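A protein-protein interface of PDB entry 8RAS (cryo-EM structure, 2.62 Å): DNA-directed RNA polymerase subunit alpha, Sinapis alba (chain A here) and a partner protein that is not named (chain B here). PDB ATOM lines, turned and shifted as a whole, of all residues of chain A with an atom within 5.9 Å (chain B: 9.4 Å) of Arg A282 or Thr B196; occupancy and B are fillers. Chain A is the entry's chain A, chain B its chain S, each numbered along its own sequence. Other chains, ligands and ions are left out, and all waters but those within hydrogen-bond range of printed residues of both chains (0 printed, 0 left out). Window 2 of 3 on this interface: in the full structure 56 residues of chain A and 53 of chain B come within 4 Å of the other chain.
OG1 of Thr B196 is in hydrogen-bond range of ND2 of Asn A285 (3.3 Å).
The backbone carbonyl oxygen (O) of Arg A282 sits at hydrogen-bond distance from the side-chain sulfur (SG) of Cys A286.
The side-chain carboxylate (OD1) of Asp A316 lies within salt-bridge range of the guanidinium group (NH2) of Arg A282, at 2.4 Å.
The backbone carbonyl oxygen (O) of Ile B193 lies within hydrogen-bond range of the side-chain hydroxyl (OG1) of Thr B196 (2.9 Å).
The side-chain amide oxygen (OE1) of Gln B289 is in hydrogen-bond range of the guanidinium group (NH2) of Arg B291.
The guanidinium group of Arg B291 is in salt-bridge range of the side-chain carboxylate of Glu B339 (3.8 Å).
The side-chain carboxylate (OD1) of Asp B335 lies within salt-bridge range of the side-chain amino group (NZ) of Lys B338 (3.2 Å).
Among the printed residues, merely in contact across the chains: Pro A281 with Ile B193 (3.6 Å), Pro A281 with Arg B291 (3.8 Å), Pro A281 with Asp B335 (3.5 Å), Arg A282 with Ile B193 (3.4 Å), Arg A282 with Thr B196 (3.8 Å), Tyr A284 with Gln B289 (3.7 Å), Tyr A284 with Arg B291 (3.4 Å), Asn A285 with Tyr B197 (3.97 Å), Asn A285 with Arg B291 (3.6 Å) and Asn A285 with Glu B339 (3.5 Å).
Of chain B, only Ile B193 (3.4 Å) and Thr B196 (3.8 Å) come within 4 Å of Arg A282.
Thr B196 touches two residues of chain A.
Of the printed residues of chain B, Pro A281 touches Ile B193, Arg B291 and Asp B335.
No residue of chain B comes within 4 Å of Ile A283.
Of the printed residues of chain A, Arg B291 touches Pro A281 (3.8 Å), Tyr A284 (3.4 Å) and Asn A285 (3.6 Å).
Of the printed residues of chain A, Gln B289 touches Tyr A284.
Printed residues of chain B within 4 Å of Tyr A284: Gln B289 and Arg B291.
Of the printed residues of chain A, Tyr B197 touches Asn A285 (3.97 Å).
Trp B199 touches none of the printed residues of chain A.
His A311 touches none of the printed residues of chain B.
The nearest residue of chain A that does not touch Thr B196 is His A311 (4.5 Å).
The nearest printed residue of chain A that does not touch Tyr B197 is Pro A281 (6.2 Å).
Printed residues of chain A that touch a printed residue of chain B: Pro A281, Arg A282, Tyr A284 and Asn A285.
Hydrophobic or aromatic side chains of chain A that line the printed part of chain B: Pro A281 and Tyr A284.
Of the 15 printed residues of chain B, 7 touch a printed residue of chain A.
Printed residues of chain B that touch a printed residue of chain A: Ile B193, Thr B196, Tyr B197, Gln B289, Arg B291, Asp B335 and Glu B339.
Along chain B the printed residues that touch a printed residue of chain A span positions 193 to 339.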
ATOM      1  N   PRO A 280      25.115  14.405  -7.678  1.00  0.00           N
ATOM      2  CA  PRO A 280      24.243  15.506  -7.281  1.00  0.00           C
ATOM      3  C   PRO A 280      25.058  16.745  -6.987  1.00  0.00           C
ATOM      4  O   PRO A 280      26.214  16.660  -6.527  1.00  0.00           O
ATOM      5  CB  PRO A 280      23.546  14.970  -6.021  1.00  0.00           C
ATOM      6  CG  PRO A 280      24.342  13.793  -5.585  1.00  0.00           C
ATOM      7  CD  PRO A 280      24.963  13.226  -6.811  1.00  0.00           C
ATOM      8  N   PRO A 281      24.503  17.933  -7.249  1.00  0.00           N
ATOM      9  CA  PRO A 281      25.294  19.165  -7.071  1.00  0.00           C
ATOM     10  C   PRO A 281      25.816  19.361  -5.658  1.00  0.00           C
ATOM     11  O   PRO A 281      26.922  19.887  -5.481  1.00  0.00           O
ATOM     12  CB  PRO A 281      24.309  20.275  -7.474  1.00  0.00           C
ATOM     13  CG  PRO A 281      22.951  19.641  -7.430  1.00  0.00           C
ATOM     14  CD  PRO A 281      23.154  18.204  -7.769  1.00  0.00           C
ATOM     15  N   ARG A 282      25.050  18.952  -4.642  1.00  0.00           N
ATOM     16  CA  ARG A 282      25.525  19.085  -3.268  1.00  0.00           C
ATOM     17  C   ARG A 282      26.771  18.242  -3.030  1.00  0.00           C
ATOM     18  O   ARG A 282      27.743  18.713  -2.427  1.00  0.00           O
ATOM     19  CB  ARG A 282      24.419  18.696  -2.289  1.00  0.00           C
ATOM     20  CG  ARG A 282      24.819  18.825  -0.827  1.00  0.00           C
ATOM     21  CD  ARG A 282      23.649  18.543   0.101  1.00  0.00           C
ATOM     22  NE  ARG A 282      23.014  17.265  -0.193  1.00  0.00           N
ATOM     23  CZ  ARG A 282      23.455  16.091   0.241  1.00  0.00           C
ATOM     24  NH1 ARG A 282      24.534  15.995   0.999  1.00  0.00           N
ATOM     25  NH2 ARG A 282      22.794  14.987  -0.095  1.00  0.00           N
ATOM     26  N   ILE A 283      26.770  16.997  -3.510  1.00  0.00           N
ATOM     27  CA  ILE A 283      27.930  16.130  -3.327  1.00  0.00           C
ATOM     28  C   ILE A 283      29.112  16.636  -4.147  1.00  0.00           C
ATOM     29  O   ILE A 283      30.266  16.564  -3.709  1.00  0.00           O
ATOM     30  CB  ILE A 283      27.570  14.675  -3.677  1.00  0.00           C
ATOM     31  CG1 ILE A 283      26.451  14.168  -2.764  1.00  0.00           C
ATOM     32  CG2 ILE A 283      28.789  13.774  -3.566  1.00  0.00           C
ATOM     33  CD1 ILE A 283      26.613  14.560  -1.310  1.00  0.00           C
ATOM     34  N   TYR A 284      28.843  17.158  -5.346  1.00  0.00           N
ATOM     35  CA  TYR A 284      29.911  17.733  -6.158  1.00  0.00           C
ATOM     36  C   TYR A 284      30.573  18.900  -5.437  1.00  0.00           C
ATOM     37  O   TYR A 284      31.804  18.992  -5.380  1.00  0.00           O
ATOM     38  CB  TYR A 284      29.357  18.172  -7.515  1.00  0.00           C
ATOM     39  CG  TYR A 284      30.381  18.794  -8.440  1.00  0.00           C
ATOM     40  CD1 TYR A 284      30.645  20.158  -8.402  1.00  0.00           C
ATOM     41  CD2 TYR A 284      31.081  18.018  -9.354  1.00  0.00           C
ATOM     42  CE1 TYR A 284      31.577  20.730  -9.243  1.00  0.00           C
ATOM     43  CE2 TYR A 284      32.015  18.582 -10.201  1.00  0.00           C
ATOM     44  CZ  TYR A 284      32.259  19.939 -10.141  1.00  0.00           C
ATOM     45  OH  TYR A 284      33.188  20.506 -10.980  1.00  0.00           O
ATOM     46  N   ASN A 285      29.766  19.799  -4.865  1.00  0.00           N
ATOM     47  CA  ASN A 285      30.322  20.924  -4.120  1.00  0.00           C
ATOM     48  C   ASN A 285      31.076  20.451  -2.883  1.00  0.00           C
ATOM     49  O   ASN A 285      32.140  20.990  -2.548  1.00  0.00           O
ATOM     50  CB  ASN A 285      29.209  21.897  -3.733  1.00  0.00           C
ATOM     51  CG  ASN A 285      28.646  22.642  -4.925  1.00  0.00           C
ATOM     52  OD1 ASN A 285      29.169  22.545  -6.034  1.00  0.00           O
ATOM     53  ND2 ASN A 285      27.572  23.390  -4.703  1.00  0.00           N
ATOM     54  N   CYS A 286      30.537  19.443  -2.191  1.00  0.00           N
ATOM     55  CA  CYS A 286      31.204  18.915  -1.005  1.00  0.00           C
ATOM     56  C   CYS A 286      32.577  18.356  -1.347  1.00  0.00           C
ATOM     57  O   CYS A 286      33.551  18.594  -0.624  1.00  0.00           O
ATOM     58  CB  CYS A 286      30.335  17.840  -0.352  1.00  0.00           C
ATOM     59  SG  CYS A 286      28.974  18.485   0.648  1.00  0.00           S
ATOM     60  N   LEU A 287      32.673  17.610  -2.448  1.00  0.00           N
ATOM     61  CA  LEU A 287      33.968  17.094  -2.877  1.00  0.00           C
ATOM     62  C   LEU A 287      34.888  18.221  -3.336  1.00  0.00           C
ATOM     63  O   LEU A 287      36.097  18.180  -3.085  1.00  0.00           O
ATOM     64  CB  LEU A 287      33.783  16.061  -3.988  1.00  0.00           C
ATOM     65  CG  LEU A 287      33.030  14.785  -3.607  1.00  0.00           C
ATOM     66  CD1 LEU A 287      32.949  13.834  -4.790  1.00  0.00           C
ATOM     67  CD2 LEU A 287      33.692  14.106  -2.419  1.00  0.00           C
ATOM     68  N   LYS A 289      35.026  21.539  -2.453  1.00  0.00           N
ATOM     69  CA  LYS A 289      35.644  22.338  -1.397  1.00  0.00           C
ATOM     70  C   LYS A 289      36.543  21.509  -0.489  1.00  0.00           C
ATOM     71  O   LYS A 289      37.328  22.087   0.272  1.00  0.00           O
ATOM     72  CB  LYS A 289      34.586  23.082  -0.568  1.00  0.00           C
ATOM     73  CG  LYS A 289      34.327  22.534   0.831  1.00  0.00           C
ATOM     74  CD  LYS A 289      33.102  23.192   1.457  1.00  0.00           C
ATOM     75  CE  LYS A 289      31.811  22.708   0.833  1.00  0.00           C
ATOM     76  NZ  LYS A 289      31.610  21.261   1.053  1.00  0.00           N
ATOM     77  N   HIS A 311      27.265  17.830   5.799  1.00  0.00           N
ATOM     78  CA  HIS A 311      26.321  17.724   4.682  1.00  0.00           C
ATOM     79  C   HIS A 311      26.529  16.444   3.868  1.00  0.00           C
ATOM     80  O   HIS A 311      26.112  16.361   2.708  1.00  0.00           O
ATOM     81  CB  HIS A 311      26.402  18.948   3.760  1.00  0.00           C
ATOM     82  CG  HIS A 311      26.519  20.255   4.486  1.00  0.00           C
ATOM     83  ND1 HIS A 311      27.246  21.315   3.988  1.00  0.00           N
ATOM     84  CD2 HIS A 311      26.001  20.677   5.665  1.00  0.00           C
ATOM     85  CE1 HIS A 311      27.175  22.330   4.829  1.00  0.00           C
ATOM     86  NE2 HIS A 311      26.426  21.969   5.855  1.00  0.00           N
ATOM     87  N   PHE A 312      27.173  15.440   4.468  1.00  0.00           N
ATOM     88  CA  PHE A 312      27.579  14.213   3.776  1.00  0.00           C
ATOM     89  C   PHE A 312      27.239  13.051   4.706  1.00  0.00           C
ATOM     90  O   PHE A 312      28.059  12.639   5.530  1.00  0.00           O
ATOM     91  CB  PHE A 312      29.061  14.247   3.425  1.00  0.00           C
ATOM     92  CG  PHE A 312      29.430  13.380   2.260  1.00  0.00           C
ATOM     93  CD1 PHE A 312      29.271  13.842   0.965  1.00  0.00           C
ATOM     94  CD2 PHE A 312      29.939  12.107   2.455  1.00  0.00           C
ATOM     95  CE1 PHE A 312      29.609  13.051  -0.114  1.00  0.00           C
ATOM     96  CE2 PHE A 312      30.279  11.310   1.377  1.00  0.00           C
ATOM     97  CZ  PHE A 312      30.114  11.783   0.091  1.00  0.00           C
ATOM     98  N   HIS A 313      26.027  12.530   4.564  1.00  0.00           N
ATOM     99  CA  HIS A 313      25.516  11.480   5.426  1.00  0.00           C
ATOM    100  C   HIS A 313      25.749  10.115   4.786  1.00  0.00           C
ATOM    101  O   HIS A 313      26.289   9.998   3.684  1.00  0.00           O
ATOM    102  CB  HIS A 313      24.032  11.716   5.721  1.00  0.00           C
ATOM    103  CG  HIS A 313      23.713  13.123   6.122  1.00  0.00           C
ATOM    104  ND1 HIS A 313      23.985  13.617   7.380  1.00  0.00           N
ATOM    105  CD2 HIS A 313      23.145  14.140   5.433  1.00  0.00           C
ATOM    106  CE1 HIS A 313      23.598  14.878   7.448  1.00  0.00           C
ATOM    107  NE2 HIS A 313      23.084  15.220   6.280  1.00  0.00           N
ATOM    108  N   ASP A 316      24.335   9.727   1.367  1.00  0.00           N
ATOM    109  CA  ASP A 316      25.229  10.252   0.341  1.00  0.00           C
ATOM    110  C   ASP A 316      26.365   9.279   0.061  1.00  0.00           C
ATOM    111  O   ASP A 316      26.751   9.082  -1.096  1.00  0.00           O
ATOM    112  CB  ASP A 316      25.780  11.611   0.771  1.00  0.00           C
ATOM    113  CG  ASP A 316      24.691  12.645   0.970  1.00  0.00           C
ATOM    114  OD1 ASP A 316      23.834  12.788   0.073  1.00  0.00           O
ATOM    115  OD2 ASP A 316      24.693  13.316   2.022  1.00  0.00           O
ATOM    116  N   LYS A 319      24.932   6.317  -1.999  1.00  0.00           N
ATOM    117  CA  LYS A 319      24.571   6.709  -3.359  1.00  0.00           C
ATOM    118  C   LYS A 319      25.811   7.017  -4.193  1.00  0.00           C
ATOM    119  O   LYS A 319      25.861   6.686  -5.384  1.00  0.00           O
ATOM    120  CB  LYS A 319      23.600   7.893  -3.335  1.00  0.00           C
ATOM    121  CG  LYS A 319      24.216   9.251  -3.051  1.00  0.00           C
ATOM    122  CD  LYS A 319      23.204  10.361  -3.280  1.00  0.00           C
ATOM    123  CE  LYS A 319      22.062  10.284  -2.281  1.00  0.00           C
ATOM    124  NZ  LYS A 319      21.032  11.331  -2.528  1.00  0.00           N
ATOM    125  N   ILE B 193      19.852  23.727  -2.290  1.00  0.00           N
ATOM    126  CA  ILE B 193      21.100  23.532  -1.564  1.00  0.00           C
ATOM    127  C   ILE B 193      21.891  24.834  -1.520  1.00  0.00           C
ATOM    128  O   ILE B 193      23.083  24.857  -1.822  1.00  0.00           O
ATOM    129  CB  ILE B 193      21.938  22.410  -2.193  1.00  0.00           C
ATOM    130  CG1 ILE B 193      21.893  22.504  -3.719  1.00  0.00           C
ATOM    131  CG2 ILE B 193      21.443  21.048  -1.728  1.00  0.00           C
ATOM    132  CD1 ILE B 193      22.923  21.648  -4.405  1.00  0.00           C
ATOM    133  N   SER B 194      21.215  25.920  -1.135  1.00  0.00           N
ATOM    134  CA  SER B 194      21.861  27.227  -1.090  1.00  0.00           C
ATOM    135  C   SER B 194      22.940  27.311  -0.020  1.00  0.00           C
ATOM    136  O   SER B 194      23.815  28.179  -0.109  1.00  0.00           O
ATOM    137  CB  SER B 194      20.817  28.320  -0.858  1.00  0.00           C
ATOM    138  OG  SER B 194      20.046  28.049   0.300  1.00  0.00           O
ATOM    139  N   HIS B 195      22.901  26.437   0.986  1.00  0.00           N
ATOM    140  CA  HIS B 195      23.905  26.459   2.042  1.00  0.00           C
ATOM    141  C   HIS B 195      25.240  25.871   1.606  1.00  0.00           C
ATOM    142  O   HIS B 195      26.234  26.043   2.318  1.00  0.00           O
ATOM    143  CB  HIS B 195      23.392  25.713   3.279  1.00  0.00           C
ATOM    144  CG  HIS B 195      22.725  24.409   2.969  1.00  0.00           C
ATOM    145  ND1 HIS B 195      23.358  23.195   3.125  1.00  0.00           N
ATOM    146  CD2 HIS B 195      21.479  24.129   2.521  1.00  0.00           C
ATOM    147  CE1 HIS B 195      22.532  22.223   2.781  1.00  0.00           C
ATOM    148  NE2 HIS B 195      21.385  22.763   2.411  1.00  0.00           N
ATOM    149  N   THR B 196      25.288  25.185   0.467  1.00  0.00           N
ATOM    150  CA  THR B 196      26.535  24.655  -0.066  1.00  0.00           C
ATOM    151  C   THR B 196      27.221  25.616  -1.028  1.00  0.00           C
ATOM    152  O   THR B 196      28.317  25.312  -1.508  1.00  0.00           O
ATOM    153  CB  THR B 196      26.288  23.317  -0.771  1.00  0.00           C
ATOM    154  OG1 THR B 196      25.674  23.551  -2.045  1.00  0.00           O
ATOM    155  CG2 THR B 196      25.381  22.433   0.072  1.00  0.00           C
ATOM    156  N   TYR B 197      26.607  26.761  -1.319  1.00  0.00           N
ATOM    157  CA  TYR B 197      27.198  27.748  -2.216  1.00  0.00           C
ATOM    158  C   TYR B 197      28.202  28.577  -1.428  1.00  0.00           C
ATOM    159  O   TYR B 197      27.823  29.340  -0.534  1.00  0.00           O
ATOM    160  CB  TYR B 197      26.119  28.634  -2.833  1.00  0.00           C
ATOM    161  CG  TYR B 197      25.088  27.895  -3.659  1.00  0.00           C
ATOM    162  CD1 TYR B 197      25.310  26.593  -4.089  1.00  0.00           C
ATOM    163  CD2 TYR B 197      23.891  28.502  -4.007  1.00  0.00           C
ATOM    164  CE1 TYR B 197      24.369  25.919  -4.840  1.00  0.00           C
ATOM    165  CE2 TYR B 197      22.944  27.836  -4.760  1.00  0.00           C
ATOM    166  CZ  TYR B 197      23.188  26.546  -5.173  1.00  0.00           C
ATOM    167  OH  TYR B 197      22.249  25.879  -5.923  1.00  0.00           O
ATOM    168  N   GLY B 198      29.481  28.434  -1.757  1.00  0.00           N
ATOM    169  CA  GLY B 198      30.547  29.098  -1.038  1.00  0.00           C
ATOM    170  C   GLY B 198      30.942  30.423  -1.652  1.00  0.00           C
ATOM    171  O   GLY B 198      30.171  31.072  -2.362  1.00  0.00           O
ATOM    172  N   TRP B 199      32.175  30.830  -1.358  1.00  0.00           N
ATOM    173  CA  TRP B 199      32.757  32.060  -1.856  1.00  0.00           C
ATOM    174  C   TRP B 199      34.069  31.759  -2.570  1.00  0.00           C
ATOM    175  O   TRP B 199      34.833  30.901  -2.115  1.00  0.00           O
ATOM    176  CB  TRP B 199      33.011  33.048  -0.710  1.00  0.00           C
ATOM    177  CG  TRP B 199      33.123  34.472  -1.145  1.00  0.00           C
ATOM    178  CD1 TRP B 199      34.267  35.199  -1.273  1.00  0.00           C
ATOM    179  CD2 TRP B 199      32.049  35.345  -1.508  1.00  0.00           C
ATOM    180  NE1 TRP B 199      33.974  36.472  -1.695  1.00  0.00           N
ATOM    181  CE2 TRP B 199      32.618  36.587  -1.847  1.00  0.00           C
ATOM    182  CE3 TRP B 199      30.661  35.197  -1.580  1.00  0.00           C
ATOM    183  CZ2 TRP B 199      31.849  37.673  -2.251  1.00  0.00           C
ATOM    184  CZ3 TRP B 199      29.900  36.275  -1.981  1.00  0.00           C
ATOM    185  CH2 TRP B 199      30.495  37.498  -2.311  1.00  0.00           C
ATOM    186  N   PRO B 200      34.362  32.435  -3.688  1.00  0.00           N
ATOM    187  CA  PRO B 200      33.577  33.482  -4.360  1.00  0.00           C
ATOM    188  C   PRO B 200      32.373  32.916  -5.106  1.00  0.00           C
ATOM    189  O   PRO B 200      32.277  31.707  -5.289  1.00  0.00           O
ATOM    190  CB  PRO B 200      34.605  34.110  -5.309  1.00  0.00           C
ATOM    191  CG  PRO B 200      35.499  32.970  -5.670  1.00  0.00           C
ATOM    192  CD  PRO B 200      35.615  32.151  -4.410  1.00  0.00           C
ATOM    193  N   LEU B 202      29.972  31.586  -7.998  1.00  0.00           N
ATOM    194  CA  LEU B 202      30.253  30.899  -9.249  1.00  0.00           C
ATOM    195  C   LEU B 202      29.851  31.763 -10.437  1.00  0.00           C
ATOM    196  O   LEU B 202      28.866  32.503 -10.384  1.00  0.00           O
ATOM    197  CB  LEU B 202      29.514  29.561  -9.294  1.00  0.00           C
ATOM    198  CG  LEU B 202      29.750  28.673 -10.517  1.00  0.00           C
ATOM    199  CD1 LEU B 202      31.106  27.996 -10.434  1.00  0.00           C
ATOM    200  CD2 LEU B 202      28.644  27.643 -10.653  1.00  0.00           C
ATOM    201  N   LYS B 263      35.713  31.607  -9.186  1.00  0.00           N
ATOM    202  CA  LYS B 263      34.998  30.367  -9.458  1.00  0.00           C
ATOM    203  C   LYS B 263      34.313  30.488 -10.813  1.00  0.00           C
ATOM    204  O   LYS B 263      33.463  31.362 -11.007  1.00  0.00           O
ATOM    205  CB  LYS B 263      33.979  30.079  -8.355  1.00  0.00           C
ATOM    206  CG  LYS B 263      33.836  28.610  -8.007  1.00  0.00           C
ATOM    207  CD  LYS B 263      32.696  28.386  -7.030  1.00  0.00           C
ATOM    208  CE  LYS B 263      33.138  28.646  -5.601  1.00  0.00           C
ATOM    209  NZ  LYS B 263      31.993  28.610  -4.651  1.00  0.00           N
ATOM    210  N   GLN B 289      35.131  24.473 -13.762  1.00  0.00           N
ATOM    211  CA  GLN B 289      34.092  23.479 -13.525  1.00  0.00           C
ATOM    212  C   GLN B 289      33.472  23.057 -14.850  1.00  0.00           C
ATOM    213  O   GLN B 289      32.840  23.866 -15.534  1.00  0.00           O
ATOM    214  CB  GLN B 289      33.029  24.038 -12.585  1.00  0.00           C
ATOM    215  CG  GLN B 289      33.497  24.197 -11.153  1.00  0.00           C
ATOM    216  CD  GLN B 289      32.382  24.622 -10.223  1.00  0.00           C
ATOM    217  OE1 GLN B 289      31.219  24.674 -10.615  1.00  0.00           O
ATOM    218  NE2 GLN B 289      32.733  24.932  -8.982  1.00  0.00           N
ATOM    219  N   ARG B 291      31.311  20.375 -15.187  1.00  0.00           N
ATOM    220  CA  ARG B 291      30.117  19.561 -15.009  1.00  0.00           C
ATOM    221  C   ARG B 291      28.961  20.038 -15.877  1.00  0.00           C
ATOM    222  O   ARG B 291      28.009  19.280 -16.091  1.00  0.00           O
ATOM    223  CB  ARG B 291      29.697  19.551 -13.540  1.00  0.00           C
ATOM    224  CG  ARG B 291      29.597  20.924 -12.912  1.00  0.00           C
ATOM    225  CD  ARG B 291      28.743  20.885 -11.661  1.00  0.00           C
ATOM    226  NE  ARG B 291      28.884  22.099 -10.867  1.00  0.00           N
ATOM    227  CZ  ARG B 291      27.990  22.523  -9.985  1.00  0.00           C
ATOM    228  NH1 ARG B 291      26.873  21.854  -9.758  1.00  0.00           N
ATOM    229  NH2 ARG B 291      28.224  23.647  -9.315  1.00  0.00           N
ATOM    230  N   ASP B 335      21.390  23.378 -12.747  1.00  0.00           N
ATOM    231  CA  ASP B 335      21.947  23.446 -11.398  1.00  0.00           C
ATOM    232  C   ASP B 335      23.039  24.506 -11.307  1.00  0.00           C
ATOM    233  O   ASP B 335      23.073  25.303 -10.359  1.00  0.00           O
ATOM    234  CB  ASP B 335      22.491  22.077 -10.991  1.00  0.00           C
ATOM    235  CG  ASP B 335      21.445  21.209 -10.324  1.00  0.00           C
ATOM    236  OD1 ASP B 335      20.835  21.662  -9.333  1.00  0.00           O
ATOM    237  OD2 ASP B 335      21.232  20.070 -10.792  1.00  0.00           O
ATOM    238  N   LYS B 338      21.465  27.909 -11.254  1.00  0.00           N
ATOM    239  CA  LYS B 338      21.014  28.316  -9.927  1.00  0.00           C
ATOM    240  C   LYS B 338      22.188  28.721  -9.047  1.00  0.00           C
ATOM    241  O   LYS B 338      22.124  29.736  -8.345  1.00  0.00           O
ATOM    242  CB  LYS B 338      20.214  27.196  -9.258  1.00  0.00           C
ATOM    243  CG  LYS B 338      19.257  26.455 -10.168  1.00  0.00           C
ATOM    244  CD  LYS B 338      18.043  25.950  -9.403  1.00  0.00           C
ATOM    245  CE  LYS B 338      17.605  24.581  -9.902  1.00  0.00           C
ATOM    246  NZ  LYS B 338      18.266  23.479  -9.150  1.00  0.00           N
ATOM    247  N   GLU B 339      23.269  27.936  -9.067  1.00  0.00           N
ATOM    248  CA  GLU B 339      24.414  28.248  -8.215  1.00  0.00           C
ATOM    249  C   GLU B 339      25.112  29.531  -8.655  1.00  0.00           C
ATOM    250  O   GLU B 339      25.513  30.342  -7.813  1.00  0.00           O
ATOM    251  CB  GLU B 339      25.402  27.083  -8.208  1.00  0.00           C
ATOM    252  CG  GLU B 339      26.614  27.326  -7.328  1.00  0.00           C
ATOM    253  CD  GLU B 339      27.521  26.119  -7.235  1.00  0.00           C
ATOM    254  OE1 GLU B 339      27.182  25.074  -7.829  1.00  0.00           O
ATOM    255  OE2 GLU B 339      28.573  26.216  -6.570  1.00  0.00           O
